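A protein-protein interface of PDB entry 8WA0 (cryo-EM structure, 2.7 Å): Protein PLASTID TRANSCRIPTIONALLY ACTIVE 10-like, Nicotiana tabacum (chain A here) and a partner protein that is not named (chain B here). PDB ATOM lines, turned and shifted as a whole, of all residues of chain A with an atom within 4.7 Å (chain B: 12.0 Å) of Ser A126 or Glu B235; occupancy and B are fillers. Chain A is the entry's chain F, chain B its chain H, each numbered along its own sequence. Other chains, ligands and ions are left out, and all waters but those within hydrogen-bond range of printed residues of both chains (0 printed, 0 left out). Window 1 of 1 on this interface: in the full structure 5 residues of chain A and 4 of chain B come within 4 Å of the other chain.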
ATOM      1  N   LYS A 123      33.912 -19.535 -10.807  1.00  0.00           N
ATOM      2  CA  LYS A 123      32.982 -19.708 -11.883  1.00  0.00           C
ATOM      3  C   LYS A 123      31.564 -19.457 -11.475  1.00  0.00           C
ATOM      4  O   LYS A 123      30.726 -19.170 -12.298  1.00  0.00           O
ATOM      5  CB  LYS A 123      33.173 -21.083 -12.473  1.00  0.00           C
ATOM      6  CG  LYS A 123      34.507 -21.279 -13.158  1.00  0.00           C
ATOM      7  CD  LYS A 123      34.707 -22.731 -13.549  1.00  0.00           C
ATOM      8  CE  LYS A 123      35.632 -22.846 -14.745  1.00  0.00           C
ATOM      9  NZ  LYS A 123      36.875 -22.049 -14.566  1.00  0.00           N
ATOM     10  N   MET A 124      31.280 -19.555 -10.198  1.00  0.00           N
ATOM     11  CA  MET A 124      29.928 -19.415  -9.715  1.00  0.00           C
ATOM     12  C   MET A 124      29.541 -18.047  -9.280  1.00  0.00           C
ATOM     13  O   MET A 124      28.468 -17.846  -8.745  1.00  0.00           O
ATOM     14  CB  MET A 124      29.671 -20.408  -8.615  1.00  0.00           C
ATOM     15  CG  MET A 124      29.546 -21.830  -9.104  1.00  0.00           C
ATOM     16  SD  MET A 124      28.082 -22.539  -8.366  1.00  0.00           S
ATOM     17  CE  MET A 124      28.507 -22.399  -6.633  1.00  0.00           C
ATOM     18  N   LEU A 125      30.384 -17.086  -9.533  1.00  0.00           N
ATOM     19  CA  LEU A 125      30.102 -15.748  -9.190  1.00  0.00           C
ATOM     20  C   LEU A 125      29.277 -15.242 -10.327  1.00  0.00           C
ATOM     21  O   LEU A 125      28.861 -14.092 -10.323  1.00  0.00           O
ATOM     22  CB  LEU A 125      31.396 -15.005  -9.040  1.00  0.00           C
ATOM     23  CG  LEU A 125      32.227 -15.059  -7.775  1.00  0.00           C
ATOM     24  CD1 LEU A 125      33.572 -14.438  -8.070  1.00  0.00           C
ATOM     25  CD2 LEU A 125      31.526 -14.300  -6.674  1.00  0.00           C
ATOM     26  N   SER A 126      29.035 -16.081 -11.319  1.00  0.00           N
ATOM     27  CA  SER A 126      28.251 -15.714 -12.472  1.00  0.00           C
ATOM     28  C   SER A 126      26.914 -16.384 -12.463  1.00  0.00           C
ATOM     29  O   SER A 126      26.828 -17.584 -12.282  1.00  0.00           O
ATOM     30  CB  SER A 126      28.982 -16.110 -13.728  1.00  0.00           C
ATOM     31  OG  SER A 126      30.187 -15.382 -13.858  1.00  0.00           O
ATOM     32  N   PRO A 127      25.851 -15.616 -12.658  1.00  0.00           N
ATOM     33  CA  PRO A 127      24.531 -16.211 -12.538  1.00  0.00           C
ATOM     34  C   PRO A 127      24.216 -17.314 -13.522  1.00  0.00           C
ATOM     35  O   PRO A 127      23.578 -18.294 -13.151  1.00  0.00           O
ATOM     36  CB  PRO A 127      23.633 -15.049 -12.775  1.00  0.00           C
ATOM     37  CG  PRO A 127      24.385 -13.883 -12.242  1.00  0.00           C
ATOM     38  CD  PRO A 127      25.799 -14.150 -12.634  1.00  0.00           C
ATOM     39  N   ASN A 128      24.648 -17.177 -14.758  1.00  0.00           N
ATOM     40  CA  ASN A 128      24.407 -18.199 -15.747  1.00  0.00           C
ATOM     41  C   ASN A 128      25.049 -19.531 -15.447  1.00  0.00           C
ATOM     42  O   ASN A 128      24.473 -20.563 -15.743  1.00  0.00           O
ATOM     43  CB  ASN A 128      24.802 -17.717 -17.121  1.00  0.00           C
ATOM     44  CG  ASN A 128      23.946 -16.564 -17.597  1.00  0.00           C
ATOM     45  OD1 ASN A 128      24.391 -15.730 -18.387  1.00  0.00           O
ATOM     46  ND2 ASN A 128      22.713 -16.502 -17.111  1.00  0.00           N
ATOM     47  N   TYR A 129      26.244 -19.540 -14.900  1.00  0.00           N
ATOM     48  CA  TYR A 129      26.899 -20.789 -14.651  1.00  0.00           C
ATOM     49  C   TYR A 129      26.056 -21.520 -13.682  1.00  0.00           C
ATOM     50  O   TYR A 129      25.873 -22.718 -13.812  1.00  0.00           O
ATOM     51  CB  TYR A 129      28.283 -20.600 -14.099  1.00  0.00           C
ATOM     52  CG  TYR A 129      29.145 -21.827 -14.046  1.00  0.00           C
ATOM     53  CD1 TYR A 129      29.104 -22.678 -12.964  1.00  0.00           C
ATOM     54  CD2 TYR A 129      30.031 -22.110 -15.062  1.00  0.00           C
ATOM     55  CE1 TYR A 129      29.900 -23.794 -12.907  1.00  0.00           C
ATOM     56  CE2 TYR A 129      30.835 -23.224 -15.013  1.00  0.00           C
ATOM     57  CZ  TYR A 129      30.766 -24.059 -13.934  1.00  0.00           C
ATOM     58  OH  TYR A 129      31.564 -25.173 -13.878  1.00  0.00           O
ATOM     59  N   ARG A 130      25.511 -20.831 -12.712  1.00  0.00           N
ATOM     60  CA  ARG A 130      24.762 -21.537 -11.718  1.00  0.00           C
ATOM     61  C   ARG A 130      23.551 -22.235 -12.283  1.00  0.00           C
ATOM     62  O   ARG A 130      23.318 -23.397 -11.977  1.00  0.00           O
ATOM     63  CB  ARG A 130      24.307 -20.580 -10.637  1.00  0.00           C
ATOM     64  CG  ARG A 130      25.345 -20.285  -9.575  1.00  0.00           C
ATOM     65  CD  ARG A 130      24.833 -19.257  -8.585  1.00  0.00           C
ATOM     66  NE  ARG A 130      24.962 -17.905  -9.102  1.00  0.00           N
ATOM     67  CZ  ARG A 130      24.667 -16.815  -8.407  1.00  0.00           C
ATOM     68  NH1 ARG A 130      24.224 -16.923  -7.165  1.00  0.00           N
ATOM     69  NH2 ARG A 130      24.818 -15.619  -8.952  1.00  0.00           N
ATOM     70  N   LYS B 229      24.408  -6.840 -28.037  1.00  0.00           N
ATOM     71  CA  LYS B 229      24.169  -6.494 -26.652  1.00  0.00           C
ATOM     72  C   LYS B 229      25.288  -6.930 -25.780  1.00  0.00           C
ATOM     73  O   LYS B 229      25.815  -8.022 -25.917  1.00  0.00           O
ATOM     74  CB  LYS B 229      22.863  -7.104 -26.163  1.00  0.00           C
ATOM     75  N   PRO B 230      25.661  -6.067 -24.866  1.00  0.00           N
ATOM     76  CA  PRO B 230      26.734  -6.372 -23.965  1.00  0.00           C
ATOM     77  C   PRO B 230      26.208  -7.215 -22.848  1.00  0.00           C
ATOM     78  O   PRO B 230      25.025  -7.501 -22.820  1.00  0.00           O
ATOM     79  CB  PRO B 230      27.115  -4.994 -23.454  1.00  0.00           C
ATOM     80  CG  PRO B 230      26.607  -4.027 -24.458  1.00  0.00           C
ATOM     81  CD  PRO B 230      25.314  -4.642 -24.843  1.00  0.00           C
ATOM     82  N   LEU B 231      27.060  -7.611 -21.915  1.00  0.00           N
ATOM     83  CA  LEU B 231      26.600  -8.374 -20.773  1.00  0.00           C
ATOM     84  C   LEU B 231      25.623  -7.576 -19.966  1.00  0.00           C
ATOM     85  O   LEU B 231      25.762  -6.375 -19.823  1.00  0.00           O
ATOM     86  CB  LEU B 231      27.744  -8.882 -19.913  1.00  0.00           C
ATOM     87  CG  LEU B 231      28.582 -10.073 -20.340  1.00  0.00           C
ATOM     88  CD1 LEU B 231      29.615 -10.355 -19.268  1.00  0.00           C
ATOM     89  CD2 LEU B 231      27.692 -11.282 -20.562  1.00  0.00           C
ATOM     90  N   THR B 232      24.613  -8.238 -19.441  1.00  0.00           N
ATOM     91  CA  THR B 232      23.584  -7.599 -18.640  1.00  0.00           C
ATOM     92  C   THR B 232      24.122  -7.275 -17.296  1.00  0.00           C
ATOM     93  O   THR B 232      25.181  -7.770 -16.928  1.00  0.00           O
ATOM     94  CB  THR B 232      22.424  -8.575 -18.452  1.00  0.00           C
ATOM     95  OG1 THR B 232      22.905  -9.766 -17.820  1.00  0.00           O
ATOM     96  CG2 THR B 232      21.812  -8.936 -19.787  1.00  0.00           C
ATOM     97  N   SER B 233      23.434  -6.461 -16.526  1.00  0.00           N
ATOM     98  CA  SER B 233      24.006  -6.044 -15.261  1.00  0.00           C
ATOM     99  C   SER B 233      24.250  -7.196 -14.349  1.00  0.00           C
ATOM    100  O   SER B 233      25.252  -7.239 -13.652  1.00  0.00           O
ATOM    101  CB  SER B 233      23.151  -5.009 -14.565  1.00  0.00           C
ATOM    102  OG  SER B 233      21.887  -5.543 -14.211  1.00  0.00           O
ATOM    103  N   GLU B 234      23.352  -8.143 -14.351  1.00  0.00           N
ATOM    104  CA  GLU B 234      23.483  -9.268 -13.489  1.00  0.00           C
ATOM    105  C   GLU B 234      24.703 -10.094 -13.762  1.00  0.00           C
ATOM    106  O   GLU B 234      25.348 -10.542 -12.823  1.00  0.00           O
ATOM    107  CB  GLU B 234      22.235 -10.112 -13.611  1.00  0.00           C
ATOM    108  CG  GLU B 234      20.946  -9.318 -13.485  1.00  0.00           C
ATOM    109  CD  GLU B 234      20.708  -8.791 -12.082  1.00  0.00           C
ATOM    110  OE1 GLU B 234      21.187  -9.417 -11.112  1.00  0.00           O
ATOM    111  OE2 GLU B 234      20.027  -7.753 -11.948  1.00  0.00           O
ATOM    112  N   GLU B 235      25.049 -10.316 -15.005  1.00  0.00           N
ATOM    113  CA  GLU B 235      26.161 -11.187 -15.308  1.00  0.00           C
ATOM    114  C   GLU B 235      27.476 -10.663 -14.843  1.00  0.00           C
ATOM    115  O   GLU B 235      28.395 -11.424 -14.636  1.00  0.00           O
ATOM    116  CB  GLU B 235      26.205 -11.490 -16.766  1.00  0.00           C
ATOM    117  CG  GLU B 235      25.832 -12.922 -17.097  1.00  0.00           C
ATOM    118  CD  GLU B 235      26.850 -13.924 -16.583  1.00  0.00           C
ATOM    119  OE1 GLU B 235      28.060 -13.721 -16.817  1.00  0.00           O
ATOM    120  OE2 GLU B 235      26.440 -14.920 -15.956  1.00  0.00           O
ATOM    121  N   LEU B 236      27.584  -9.360 -14.700  1.00  0.00           N
ATOM    122  CA  LEU B 236      28.818  -8.745 -14.309  1.00  0.00           C
ATOM    123  C   LEU B 236      29.175  -9.021 -12.910  1.00  0.00           C
ATOM    124  O   LEU B 236      28.320  -9.286 -12.093  1.00  0.00           O
ATOM    125  CB  LEU B 236      28.758  -7.254 -14.586  1.00  0.00           C
ATOM    126  CG  LEU B 236      28.606  -6.803 -16.025  1.00  0.00           C
ATOM    127  CD1 LEU B 236      28.510  -5.293 -16.061  1.00  0.00           C
ATOM    128  CD2 LEU B 236      29.783  -7.289 -16.850  1.00  0.00           C
ATOM    129  N   TRP B 237      30.438  -8.944 -12.607  1.00  0.00           N
ATOM    130  CA  TRP B 237      30.920  -9.199 -11.299  1.00  0.00           C
ATOM    131  C   TRP B 237      30.493  -8.087 -10.418  1.00  0.00           C
ATOM    132  O   TRP B 237      30.161  -7.014 -10.904  1.00  0.00           O
ATOM    133  CB  TRP B 237      32.412  -9.241 -11.301  1.00  0.00           C
ATOM    134  CG  TRP B 237      33.103 -10.405 -11.847  1.00  0.00           C
ATOM    135  CD1 TRP B 237      32.728 -11.698 -11.768  1.00  0.00           C
ATOM    136  CD2 TRP B 237      34.366 -10.389 -12.505  1.00  0.00           C
ATOM    137  NE1 TRP B 237      33.666 -12.493 -12.365  1.00  0.00           N
ATOM    138  CE2 TRP B 237      34.683 -11.705 -12.825  1.00  0.00           C
ATOM    139  CE3 TRP B 237      35.254  -9.378 -12.866  1.00  0.00           C
ATOM    140  CZ2 TRP B 237      35.841 -12.041 -13.487  1.00  0.00           C
ATOM    141  CZ3 TRP B 237      36.401  -9.719 -13.520  1.00  0.00           C
ATOM    142  CH2 TRP B 237      36.686 -11.035 -13.825  1.00  0.00           C
ATOM    143  N   TRP B 238      30.527  -8.275  -9.123  1.00  0.00           N
ATOM    144  CA  TRP B 238      29.994  -7.318  -8.174  1.00  0.00           C
ATOM    145  C   TRP B 238      30.594  -5.979  -8.190  1.00  0.00           C
ATOM    146  O   TRP B 238      29.909  -4.997  -8.009  1.00  0.00           O
ATOM    147  CB  TRP B 238      30.050  -7.922  -6.791  1.00  0.00           C
ATOM    148  CG  TRP B 238      31.292  -7.776  -5.959  1.00  0.00           C
ATOM    149  CD1 TRP B 238      31.701  -6.672  -5.265  1.00  0.00           C
ATOM    150  CD2 TRP B 238      32.230  -8.799  -5.656  1.00  0.00           C
ATOM    151  NE1 TRP B 238      32.858  -6.936  -4.591  1.00  0.00           N
ATOM    152  CE2 TRP B 238      33.202  -8.241  -4.815  1.00  0.00           C
ATOM    153  CE3 TRP B 238      32.357 -10.131  -6.036  1.00  0.00           C
ATOM    154  CZ2 TRP B 238      34.281  -8.968  -4.344  1.00  0.00           C
ATOM    155  CZ3 TRP B 238      33.425 -10.855  -5.566  1.00  0.00           C
ATOM    156  CH2 TRP B 238      34.378 -10.272  -4.732  1.00  0.00           C
ATOM    157  N   ASN B 239      31.871  -5.910  -8.405  1.00  0.00           N
ATOM    158  CA  ASN B 239      32.566  -4.676  -8.367  1.00  0.00           C
ATOM    159  C   ASN B 239      32.030  -3.760  -9.403  1.00  0.00           C
ATOM    160  O   ASN B 239      32.077  -2.561  -9.232  1.00  0.00           O
ATOM    161  CB  ASN B 239      34.082  -4.937  -8.513  1.00  0.00           C
ATOM    162  CG  ASN B 239      34.431  -5.948  -9.571  1.00  0.00           C
ATOM    163  OD1 ASN B 239      33.571  -6.527 -10.223  1.00  0.00           O
ATOM    164  ND2 ASN B 239      35.719  -6.163  -9.755  1.00  0.00           N
ATOM    165  N   TRP B 240      31.517  -4.293 -10.490  1.00  0.00           N
ATOM    166  CA  TRP B 240      31.120  -3.501 -11.611  1.00  0.00           C
ATOM    167  C   TRP B 240      29.663  -3.381 -11.802  1.00  0.00           C
ATOM    168  O   TRP B 240      29.215  -3.077 -12.887  1.00  0.00           O
ATOM    169  CB  TRP B 240      31.708  -4.135 -12.850  1.00  0.00           C
ATOM    170  CG  TRP B 240      33.170  -4.092 -13.027  1.00  0.00           C
ATOM    171  CD1 TRP B 240      34.021  -5.134 -12.929  1.00  0.00           C
ATOM    172  CD2 TRP B 240      33.959  -2.964 -13.399  1.00  0.00           C
ATOM    173  NE1 TRP B 240      35.296  -4.732 -13.191  1.00  0.00           N
ATOM    174  CE2 TRP B 240      35.286  -3.398 -13.482  1.00  0.00           C
ATOM    175  CE3 TRP B 240      33.672  -1.626 -13.659  1.00  0.00           C
ATOM    176  CZ2 TRP B 240      36.324  -2.548 -13.813  1.00  0.00           C
ATOM    177  CZ3 TRP B 240      34.700  -0.785 -13.985  1.00  0.00           C
ATOM    178  CH2 TRP B 240      36.011  -1.246 -14.062  1.00  0.00           C
ATOM    179  N   ARG B 241      28.893  -3.626 -10.780  1.00  0.00           N
ATOM    180  CA  ARG B 241      27.489  -3.656 -10.935  1.00  0.00           C
ATOM    181  C   ARG B 241      26.877  -2.413 -10.407  1.00  0.00           C
ATOM    182  O   ARG B 241      27.152  -2.013  -9.296  1.00  0.00           O
ATOM    183  CB  ARG B 241      26.934  -4.931 -10.309  1.00  0.00           C
ATOM    184  CG  ARG B 241      25.639  -5.424 -10.895  1.00  0.00           C
ATOM    185  CD  ARG B 241      25.178  -6.659 -10.151  1.00  0.00           C
ATOM    186  NE  ARG B 241      26.240  -7.643 -10.030  1.00  0.00           N
ATOM    187  CZ  ARG B 241      26.109  -8.797  -9.391  1.00  0.00           C
ATOM    188  NH1 ARG B 241      24.964  -9.105  -8.814  1.00  0.00           N
ATOM    189  NH2 ARG B 241      27.123  -9.640  -9.325  1.00  0.00           N
ATOM    190  N   LYS B 242      26.055  -1.776 -11.208  1.00  0.00           N
ATOM    191  CA  LYS B 242      25.417  -0.536 -10.858  1.00  0.00           C
ATOM    192  C   LYS B 242      24.406  -0.700  -9.822  1.00  0.00           C
ATOM    193  O   LYS B 242      23.687  -1.686  -9.805  1.00  0.00           O
ATOM    194  CB  LYS B 242      24.720   0.013 -12.087  1.00  0.00           C
ATOM    195  CG  LYS B 242      25.187   1.388 -12.514  1.00  0.00           C
ATOM    196  CD  LYS B 242      24.136   2.065 -13.376  1.00  0.00           C
ATOM    197  CE  LYS B 242      22.811   2.180 -12.634  1.00  0.00           C
ATOM    198  NZ  LYS B 242      22.931   2.969 -11.377  1.00  0.00           N
ATOM    199  N   GLU B 244      21.061  -0.502  -7.590  1.00  0.00           N
ATOM    200  CA  GLU B 244      19.671  -0.545  -8.015  1.00  0.00           C
ATOM    201  C   GLU B 244      18.958   0.762  -7.834  1.00  0.00           C
ATOM    202  O   GLU B 244      18.075   1.099  -8.608  1.00  0.00           O
ATOM    203  CB  GLU B 244      18.930  -1.606  -7.224  1.00  0.00           C
ATOM    204  CG  GLU B 244      19.637  -2.951  -7.177  1.00  0.00           C
ATOM    205  CD  GLU B 244      19.623  -3.678  -8.508  1.00  0.00           C
ATOM    206  OE1 GLU B 244      18.701  -3.439  -9.317  1.00  0.00           O
ATOM    207  OE2 GLU B 244      20.530  -4.503  -8.742  1.00  0.00           O
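Printed residues of chain B that touch a printed residue of chain A: Glu B234 and Glu B235. Hydrophobic or aromatic side chains of chain A within 4 Å of the printed part of chain B: Pro A127.
Of chain B, only Glu B235 comes within 4 Å of Ser A126. Of chain B, only Glu B235 comes within 4 Å of Asn A128. No residue of chain B comes within 4 Å of Arg A130. Printed residues of chain A within 4 Å of Glu B234: Pro A127. The nearest residue of chain B that does not touch Ser A126 is Trp B237 (4.8 Å). The nearest printed residue of chain A that does not touch Glu B235 is Tyr A129 (4.7 Å). The nearest printed residue of chain A that does not touch Glu B234 is Leu A125 (5.6 Å).
Among the printed residues, pairs that only touch across the chains: Pro A127 with Glu B234 (3.5 Å) and Ser A126 with Glu B235 (3.6 Å).
The backbone NH of Asn A128 is in hydrogen-bond range of the side-chain carboxylate of Glu B235. The backbone nitrogen of Pro A127 sits close to the side-chain carboxylate of Glu B235 (3.4 Å).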
